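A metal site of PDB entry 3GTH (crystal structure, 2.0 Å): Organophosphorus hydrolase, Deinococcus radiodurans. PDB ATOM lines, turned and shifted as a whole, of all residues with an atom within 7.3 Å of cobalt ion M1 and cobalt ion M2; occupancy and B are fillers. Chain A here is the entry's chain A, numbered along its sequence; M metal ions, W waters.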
ATOM      1  N   HIS A  35      -1.432  -3.045  24.415  1.00  0.00           N
ATOM      2  CA  HIS A  35      -2.079  -4.256  24.936  1.00  0.00           C
ATOM      3  C   HIS A  35      -1.097  -5.400  25.146  1.00  0.00           C
ATOM      4  O   HIS A  35      -0.775  -6.119  24.216  1.00  0.00           O
ATOM      5  CB  HIS A  35      -3.197  -4.702  23.981  1.00  0.00           C
ATOM      6  CG  HIS A  35      -4.027  -5.832  24.517  1.00  0.00           C
ATOM      7  ND1 HIS A  35      -5.406  -5.801  24.506  1.00  0.00           N
ATOM      8  CD2 HIS A  35      -3.678  -7.036  25.034  1.00  0.00           C
ATOM      9  CE1 HIS A  35      -5.862  -6.943  24.998  1.00  0.00           C
ATOM     10  NE2 HIS A  35      -4.834  -7.710  25.325  1.00  0.00           N
ATOM     11  N   GLU A  36      -0.631  -5.526  26.374  1.00  0.00           N
ATOM     12  CA  GLU A  36       0.286  -6.595  26.795  1.00  0.00           C
ATOM     13  C   GLU A  36      -0.096  -7.082  28.203  1.00  0.00           C
ATOM     14  O   GLU A  36      -0.952  -6.517  28.889  1.00  0.00           O
ATOM     15  CB  GLU A  36       1.727  -6.077  26.857  1.00  0.00           C
ATOM     16  CG  GLU A  36       2.201  -5.270  25.611  1.00  0.00           C
ATOM     17  CD  GLU A  36       2.322  -6.135  24.368  1.00  0.00           C
ATOM     18  OE1 GLU A  36       2.217  -5.616  23.241  1.00  0.00           O
ATOM     19  OE2 GLU A  36       2.547  -7.353  24.515  1.00  0.00           O
ATOM     20  N   HIS A  37       0.560  -8.158  28.628  1.00  0.00           N
ATOM     21  CA  HIS A  37       0.318  -8.717  29.939  1.00  0.00           C
ATOM     22  C   HIS A  37       1.647  -9.075  30.591  1.00  0.00           C
ATOM     23  O   HIS A  37       2.295 -10.061  30.174  1.00  0.00           O
ATOM     24  CB  HIS A  37      -0.499  -9.987  29.778  1.00  0.00           C
ATOM     25  CG  HIS A  37      -1.836  -9.760  29.187  1.00  0.00           C
ATOM     26  ND1 HIS A  37      -2.892  -9.231  29.925  1.00  0.00           N
ATOM     27  CD2 HIS A  37      -2.332  -9.977  27.943  1.00  0.00           C
ATOM     28  CE1 HIS A  37      -3.948  -9.146  29.157  1.00  0.00           C
ATOM     29  NE2 HIS A  37      -3.635  -9.583  27.954  1.00  0.00           N
ATOM     30  N   PHE A  40      -0.025 -13.155  33.641  1.00  0.00           N
ATOM     31  CA  PHE A  40      -1.358 -13.511  33.255  1.00  0.00           C
ATOM     32  C   PHE A  40      -1.656 -14.976  33.536  1.00  0.00           C
ATOM     33  O   PHE A  40      -0.799 -15.836  33.391  1.00  0.00           O
ATOM     34  CB  PHE A  40      -1.548 -13.229  31.773  1.00  0.00           C
ATOM     35  CG  PHE A  40      -2.927 -13.567  31.251  1.00  0.00           C
ATOM     36  CD1 PHE A  40      -3.265 -14.886  30.940  1.00  0.00           C
ATOM     37  CD2 PHE A  40      -3.904 -12.549  31.102  1.00  0.00           C
ATOM     38  CE1 PHE A  40      -4.522 -15.227  30.486  1.00  0.00           C
ATOM     39  CE2 PHE A  40      -5.193 -12.884  30.645  1.00  0.00           C
ATOM     40  CZ  PHE A  40      -5.500 -14.231  30.332  1.00  0.00           C
ATOM     41  N   ALA A  81      -3.359  -5.046  29.940  1.00  0.00           N
ATOM     42  CA  ALA A  81      -4.787  -5.274  29.748  1.00  0.00           C
ATOM     43  C   ALA A  81      -5.382  -6.451  30.530  1.00  0.00           C
ATOM     44  O   ALA A  81      -6.454  -6.963  30.196  1.00  0.00           O
ATOM     45  CB  ALA A  81      -5.043  -5.473  28.240  1.00  0.00           C
ATOM     46  N   THR A  82      -4.677  -6.872  31.554  1.00  0.00           N
ATOM     47  CA  THR A  82      -5.118  -8.023  32.318  1.00  0.00           C
ATOM     48  C   THR A  82      -6.373  -7.766  33.129  1.00  0.00           C
ATOM     49  O   THR A  82      -6.403  -6.894  33.979  1.00  0.00           O
ATOM     50  CB  THR A  82      -4.015  -8.492  33.269  1.00  0.00           C
ATOM     51  OG1 THR A  82      -2.781  -8.519  32.550  1.00  0.00           O
ATOM     52  CG2 THR A  82      -4.335  -9.910  33.799  1.00  0.00           C
ATOM     53  N   PRO A  83      -7.413  -8.558  32.892  1.00  0.00           N
ATOM     54  CA  PRO A  83      -8.719  -8.492  33.564  1.00  0.00           C
ATOM     55  C   PRO A  83      -8.546  -8.823  35.021  1.00  0.00           C
ATOM     56  O   PRO A  83      -7.630  -9.571  35.404  1.00  0.00           O
ATOM     57  CB  PRO A  83      -9.540  -9.533  32.848  1.00  0.00           C
ATOM     58  CG  PRO A  83      -8.964  -9.548  31.522  1.00  0.00           C
ATOM     59  CD  PRO A  83      -7.500  -9.360  31.661  1.00  0.00           C
ATOM     60  N   TYR A 111     -13.158 -10.428  32.081  1.00  0.00           N
ATOM     61  CA  TYR A 111     -13.009 -10.946  30.738  1.00  0.00           C
ATOM     62  C   TYR A 111     -14.328 -11.382  30.128  1.00  0.00           C
ATOM     63  O   TYR A 111     -15.340 -11.345  30.789  1.00  0.00           O
ATOM     64  CB  TYR A 111     -12.000 -12.146  30.768  1.00  0.00           C
ATOM     65  CG  TYR A 111     -11.087 -12.223  29.567  1.00  0.00           C
ATOM     66  CD1 TYR A 111     -10.956 -11.120  28.722  1.00  0.00           C
ATOM     67  CD2 TYR A 111     -10.269 -13.337  29.327  1.00  0.00           C
ATOM     68  CE1 TYR A 111     -10.063 -11.100  27.680  1.00  0.00           C
ATOM     69  CE2 TYR A 111      -9.352 -13.309  28.265  1.00  0.00           C
ATOM     70  CZ  TYR A 111      -9.260 -12.188  27.451  1.00  0.00           C
ATOM     71  OH  TYR A 111      -8.373 -12.079  26.422  1.00  0.00           O
ATOM     72  N   TYR A 112     -14.304 -11.789  28.866  1.00  0.00           N
ATOM     73  CA  TYR A 112     -15.486 -12.245  28.157  1.00  0.00           C
ATOM     74  C   TYR A 112     -16.080 -13.499  28.798  1.00  0.00           C
ATOM     75  O   TYR A 112     -15.392 -14.264  29.485  1.00  0.00           O
ATOM     76  CB  TYR A 112     -15.180 -12.460  26.662  1.00  0.00           C
ATOM     77  CG  TYR A 112     -14.371 -13.693  26.267  1.00  0.00           C
ATOM     78  CD1 TYR A 112     -14.963 -14.755  25.575  1.00  0.00           C
ATOM     79  CD2 TYR A 112     -13.004 -13.797  26.580  1.00  0.00           C
ATOM     80  CE1 TYR A 112     -14.249 -15.873  25.212  1.00  0.00           C
ATOM     81  CE2 TYR A 112     -12.269 -14.933  26.215  1.00  0.00           C
ATOM     82  CZ  TYR A 112     -12.900 -15.965  25.538  1.00  0.00           C
ATOM     83  OH  TYR A 112     -12.225 -17.117  25.192  1.00  0.00           O
ATOM     84  N   KCX A 157     -11.015  -2.359  30.806  1.00  0.00           N
ATOM     85  CA  KCX A 157     -10.904  -3.398  29.796  1.00  0.00           C
ATOM     86  CB  KCX A 157      -9.830  -4.439  30.234  1.00  0.00           C
ATOM     87  CG  KCX A 157      -9.840  -5.810  29.467  1.00  0.00           C
ATOM     88  CD  KCX A 157      -9.335  -5.643  28.067  1.00  0.00           C
ATOM     89  CE  KCX A 157      -9.216  -7.011  27.379  1.00  0.00           C
ATOM     90  NZ  KCX A 157      -8.050  -7.736  27.840  1.00  0.00           N
ATOM     91  C   KCX A 157     -12.278  -4.037  29.648  1.00  0.00           C
ATOM     92  O   KCX A 157     -12.865  -4.486  30.598  1.00  0.00           O
ATOM     93  CX  KCX A 157      -7.493  -8.748  27.172  1.00  0.00           C
ATOM     94  OQ1 KCX A 157      -7.925  -9.103  26.064  1.00  0.00           O
ATOM     95  OQ2 KCX A 157      -6.495  -9.353  27.631  1.00  0.00           O
ATOM     96  N   LEU A 158     -12.791  -4.052  28.445  1.00  0.00           N
ATOM     97  CA  LEU A 158     -14.067  -4.670  28.175  1.00  0.00           C
ATOM     98  C   LEU A 158     -13.769  -5.821  27.217  1.00  0.00           C
ATOM     99  O   LEU A 158     -12.772  -5.775  26.482  1.00  0.00           O
ATOM    100  CB  LEU A 158     -14.997  -3.666  27.463  1.00  0.00           C
ATOM    101  CG  LEU A 158     -15.481  -2.449  28.255  1.00  0.00           C
ATOM    102  CD1 LEU A 158     -16.379  -1.546  27.343  1.00  0.00           C
ATOM    103  CD2 LEU A 158     -16.258  -2.968  29.474  1.00  0.00           C
ATOM    104  N   ALA A 159     -14.654  -6.822  27.180  1.00  0.00           N
ATOM    105  CA  ALA A 159     -14.475  -7.982  26.264  1.00  0.00           C
ATOM    106  C   ALA A 159     -15.823  -8.590  25.860  1.00  0.00           C
ATOM    107  O   ALA A 159     -16.754  -8.639  26.640  1.00  0.00           O
ATOM    108  CB  ALA A 159     -13.585  -9.072  26.904  1.00  0.00           C
ATOM    109  N   THR A 189     -10.580  -2.848  24.430  1.00  0.00           N
ATOM    110  CA  THR A 189     -11.370  -4.044  24.442  1.00  0.00           C
ATOM    111  C   THR A 189     -10.743  -5.268  23.821  1.00  0.00           C
ATOM    112  O   THR A 189      -9.703  -5.178  23.184  1.00  0.00           O
ATOM    113  CB  THR A 189     -12.664  -3.824  23.695  1.00  0.00           C
ATOM    114  OG1 THR A 189     -12.431  -4.030  22.306  1.00  0.00           O
ATOM    115  CG2 THR A 189     -13.141  -2.397  23.910  1.00  0.00           C
ATOM    116  N   HIS A 190     -11.446  -6.385  24.023  1.00  0.00           N
ATOM    117  CA  HIS A 190     -11.138  -7.698  23.487  1.00  0.00           C
ATOM    118  C   HIS A 190     -12.304  -8.082  22.567  1.00  0.00           C
ATOM    119  O   HIS A 190     -13.472  -7.972  22.955  1.00  0.00           O
ATOM    120  CB  HIS A 190     -11.048  -8.726  24.630  1.00  0.00           C
ATOM    121  CG  HIS A 190     -11.145 -10.161  24.196  1.00  0.00           C
ATOM    122  ND1 HIS A 190     -10.115 -11.066  24.345  1.00  0.00           N
ATOM    123  CD2 HIS A 190     -12.196 -10.877  23.717  1.00  0.00           C
ATOM    124  CE1 HIS A 190     -10.523 -12.267  23.981  1.00  0.00           C
ATOM    125  NE2 HIS A 190     -11.770 -12.185  23.599  1.00  0.00           N
ATOM    126  N   THR A 191     -11.999  -8.495  21.364  1.00  0.00           N
ATOM    127  CA  THR A 191     -13.032  -9.010  20.486  1.00  0.00           C
ATOM    128  C   THR A 191     -12.562 -10.446  20.319  1.00  0.00           C
ATOM    129  O   THR A 191     -11.369 -10.691  20.194  1.00  0.00           O
ATOM    130  CB  THR A 191     -13.104  -8.353  19.097  1.00  0.00           C
ATOM    131  OG1 THR A 191     -11.808  -8.370  18.475  1.00  0.00           O
ATOM    132  CG2 THR A 191     -13.677  -6.935  19.234  1.00  0.00           C
ATOM    133  N   GLN A 192     -13.503 -11.365  20.359  1.00  0.00           N
ATOM    134  CA  GLN A 192     -13.237 -12.791  20.265  1.00  0.00           C
ATOM    135  C   GLN A 192     -13.304 -13.260  18.824  1.00  0.00           C
ATOM    136  O   GLN A 192     -14.292 -13.038  18.133  1.00  0.00           O
ATOM    137  CB  GLN A 192     -14.278 -13.523  21.082  1.00  0.00           C
ATOM    138  CG  GLN A 192     -14.065 -15.012  21.242  1.00  0.00           C
ATOM    139  CD  GLN A 192     -12.726 -15.355  21.840  1.00  0.00           C
ATOM    140  OE1 GLN A 192     -12.118 -14.557  22.599  1.00  0.00           O
ATOM    141  NE2 GLN A 192     -12.245 -16.546  21.517  1.00  0.00           N
ATOM    142  N   GLY A 217     -10.047  -3.720  20.446  1.00  0.00           N
ATOM    143  CA  GLY A 217      -8.939  -4.668  20.269  1.00  0.00           C
ATOM    144  C   GLY A 217      -9.156  -5.930  19.465  1.00  0.00           C
ATOM    145  O   GLY A 217     -10.271  -6.273  19.049  1.00  0.00           O
ATOM    146  N   HIS A 218      -8.036  -6.641  19.289  1.00  0.00           N
ATOM    147  CA  HIS A 218      -7.954  -7.886  18.517  1.00  0.00           C
ATOM    148  C   HIS A 218      -8.620  -7.745  17.175  1.00  0.00           C
ATOM    149  O   HIS A 218      -9.151  -8.734  16.635  1.00  0.00           O
ATOM    150  CB  HIS A 218      -8.520  -9.092  19.280  1.00  0.00           C
ATOM    151  CG  HIS A 218      -8.030  -9.222  20.686  1.00  0.00           C
ATOM    152  ND1 HIS A 218      -6.871  -8.616  21.132  1.00  0.00           N
ATOM    153  CD2 HIS A 218      -8.586  -9.794  21.791  1.00  0.00           C
ATOM    154  CE1 HIS A 218      -6.747  -8.792  22.433  1.00  0.00           C
ATOM    155  NE2 HIS A 218      -7.777  -9.501  22.858  1.00  0.00           N
ATOM    156  N   ASP A 241      -3.526  -6.080  17.810  1.00  0.00           N
ATOM    157  CA  ASP A 241      -2.785  -6.268  19.031  1.00  0.00           C
ATOM    158  C   ASP A 241      -2.391  -7.662  19.445  1.00  0.00           C
ATOM    159  O   ASP A 241      -2.057  -7.870  20.598  1.00  0.00           O
ATOM    160  CB  ASP A 241      -3.522  -5.560  20.149  1.00  0.00           C
ATOM    161  CG  ASP A 241      -4.951  -6.054  20.311  1.00  0.00           C
ATOM    162  OD1 ASP A 241      -5.737  -5.332  20.957  1.00  0.00           O
ATOM    163  OD2 ASP A 241      -5.274  -7.162  19.787  1.00  0.00           O
ATOM    164  N   ARG A 242      -2.458  -8.596  18.505  1.00  0.00           N
ATOM    165  CA  ARG A 242      -2.009  -9.963  18.772  1.00  0.00           C
ATOM    166  C   ARG A 242      -0.939 -10.306  17.694  1.00  0.00           C
ATOM    167  O   ARG A 242      -0.870 -11.432  17.195  1.00  0.00           O
ATOM    168  CB  ARG A 242      -3.182 -10.934  18.676  1.00  0.00           C
ATOM    169  CG  ARG A 242      -4.407 -10.474  19.489  1.00  0.00           C
ATOM    170  CD  ARG A 242      -5.430 -11.583  19.560  1.00  0.00           C
ATOM    171  NE  ARG A 242      -5.210 -12.371  20.763  1.00  0.00           N
ATOM    172  CZ  ARG A 242      -5.634 -13.611  20.938  1.00  0.00           C
ATOM    173  NH1 ARG A 242      -6.309 -14.217  19.981  1.00  0.00           N
ATOM    174  NH2 ARG A 242      -5.392 -14.242  22.081  1.00  0.00           N
ATOM    175  N   HIS A 277       1.132  -6.865  20.809  1.00  0.00           N
ATOM    176  CA  HIS A 277       1.372  -8.321  20.732  1.00  0.00           C
ATOM    177  C   HIS A 277       0.402  -9.176  21.555  1.00  0.00           C
ATOM    178  O   HIS A 277       0.172 -10.350  21.235  1.00  0.00           O
ATOM    179  CB  HIS A 277       2.799  -8.667  21.240  1.00  0.00           C
ATOM    180  CG  HIS A 277       3.884  -7.733  20.777  1.00  0.00           C
ATOM    181  ND1 HIS A 277       4.564  -7.915  19.590  1.00  0.00           N
ATOM    182  CD2 HIS A 277       4.385  -6.607  21.323  1.00  0.00           C
ATOM    183  CE1 HIS A 277       5.433  -6.942  19.427  1.00  0.00           C
ATOM    184  NE2 HIS A 277       5.341  -6.129  20.467  1.00  0.00           N
ATOM    185  N   ASP A 278      -0.101  -8.618  22.636  1.00  0.00           N
ATOM    186  CA  ASP A 278      -1.014  -9.360  23.551  1.00  0.00           C
ATOM    187  C   ASP A 278      -0.147 -10.475  24.184  1.00  0.00           C
ATOM    188  O   ASP A 278      -0.631 -11.563  24.477  1.00  0.00           O
ATOM    189  CB  ASP A 278      -2.171 -10.008  22.770  1.00  0.00           C
ATOM    190  CG  ASP A 278      -3.254 -10.515  23.676  1.00  0.00           C
ATOM    191  OD1 ASP A 278      -4.160 -11.250  23.223  1.00  0.00           O
ATOM    192  OD2 ASP A 278      -3.190 -10.175  24.869  1.00  0.00           O
ATOM    193  N   SER A 279       1.124 -10.188  24.360  1.00  0.00           N
ATOM    194  CA  SER A 279       2.042 -11.186  24.875  1.00  0.00           C
ATOM    195  C   SER A 279       1.883 -11.361  26.379  1.00  0.00           C
ATOM    196  O   SER A 279       1.285 -10.514  27.056  1.00  0.00           O
ATOM    197  CB  SER A 279       3.499 -10.737  24.573  1.00  0.00           C
ATOM    198  OG  SER A 279       3.924  -9.647  25.379  1.00  0.00           O
ATOM    199  N   ILE A 280       2.411 -12.470  26.895  1.00  0.00           N
ATOM    200  CA  ILE A 280       2.392 -12.707  28.326  1.00  0.00           C
ATOM    201  C   ILE A 280       3.864 -12.920  28.710  1.00  0.00           C
ATOM    202  O   ILE A 280       4.524 -13.848  28.247  1.00  0.00           O
ATOM    203  CB  ILE A 280       1.488 -13.898  28.652  1.00  0.00           C
ATOM    204  CG1 ILE A 280       0.039 -13.497  28.416  1.00  0.00           C
ATOM    205  CG2 ILE A 280       1.693 -14.331  30.089  1.00  0.00           C
ATOM    206  CD1 ILE A 280      -0.864 -14.645  27.954  1.00  0.00           C
HETATM  207 CO    CO M   1      -8.047 -10.574  24.786  1.00  0.00          CO
HETATM  208 CO    CO M   2      -4.924  -9.573  26.266  1.00  0.00          CO
HETATM  209  O   HOH W   1      -7.738 -12.475  23.700  1.00  0.00           O
HETATM  210  O   HOH W   2      -5.824 -10.689  25.250  1.00  0.00           O
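NZ of KCX 157 sits close to the backbone carbonyl oxygen (O) of Ala 81 (2.9 Å). ND1 of His 37 lies within hydrogen-bond range of OG1 of Thr 82. The backbone NH of His 37 is in hydrogen-bond range of the backbone carbonyl oxygen of Ser 279, at 2.9 Å. N of His 190 is in hydrogen-bond range of O of Leu 158, at 2.9 Å. The backbone carbonyl oxygen (O) of His 218 sits at hydrogen-bond distance from the side-chain hydroxyl (OG1) of Thr 191 (3.3 Å). The side-chain carboxylate of Asp 278 is in salt-bridge range of the guanidinium group of Arg 242 (2.9 Å). OE2 of Glu 36 lies within hydrogen-bond range of N of Asp 278 (3.5 Å). The backbone NH (N) of Asp 278 is in hydrogen-bond range of the backbone carbonyl oxygen (O) of Asp 241, at 2.9 Å.
Within 4 Å of cobalt ion M2: His 35, His 37, KCX 157 and Asp 278.
Cobalt ion M1 is bound by OQ1 of KCX 157 (2.0 Å), ND1 of His 190 (2.2 Å), water W1 (2.2 Å), NE2 of His 218 (2.2 Å), OH of Tyr 111 (2.2 Å) and water W2 (2.3 Å).
Cobalt ion M2 is bound by water W2, a ring nitrogen (NE2) of His 35, OQ2 of KCX 157, a ring nitrogen (NE2) of His 37 and the side-chain carboxylate of Asp 278. Cobalt ion M2 has five donor atoms within binding distance.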
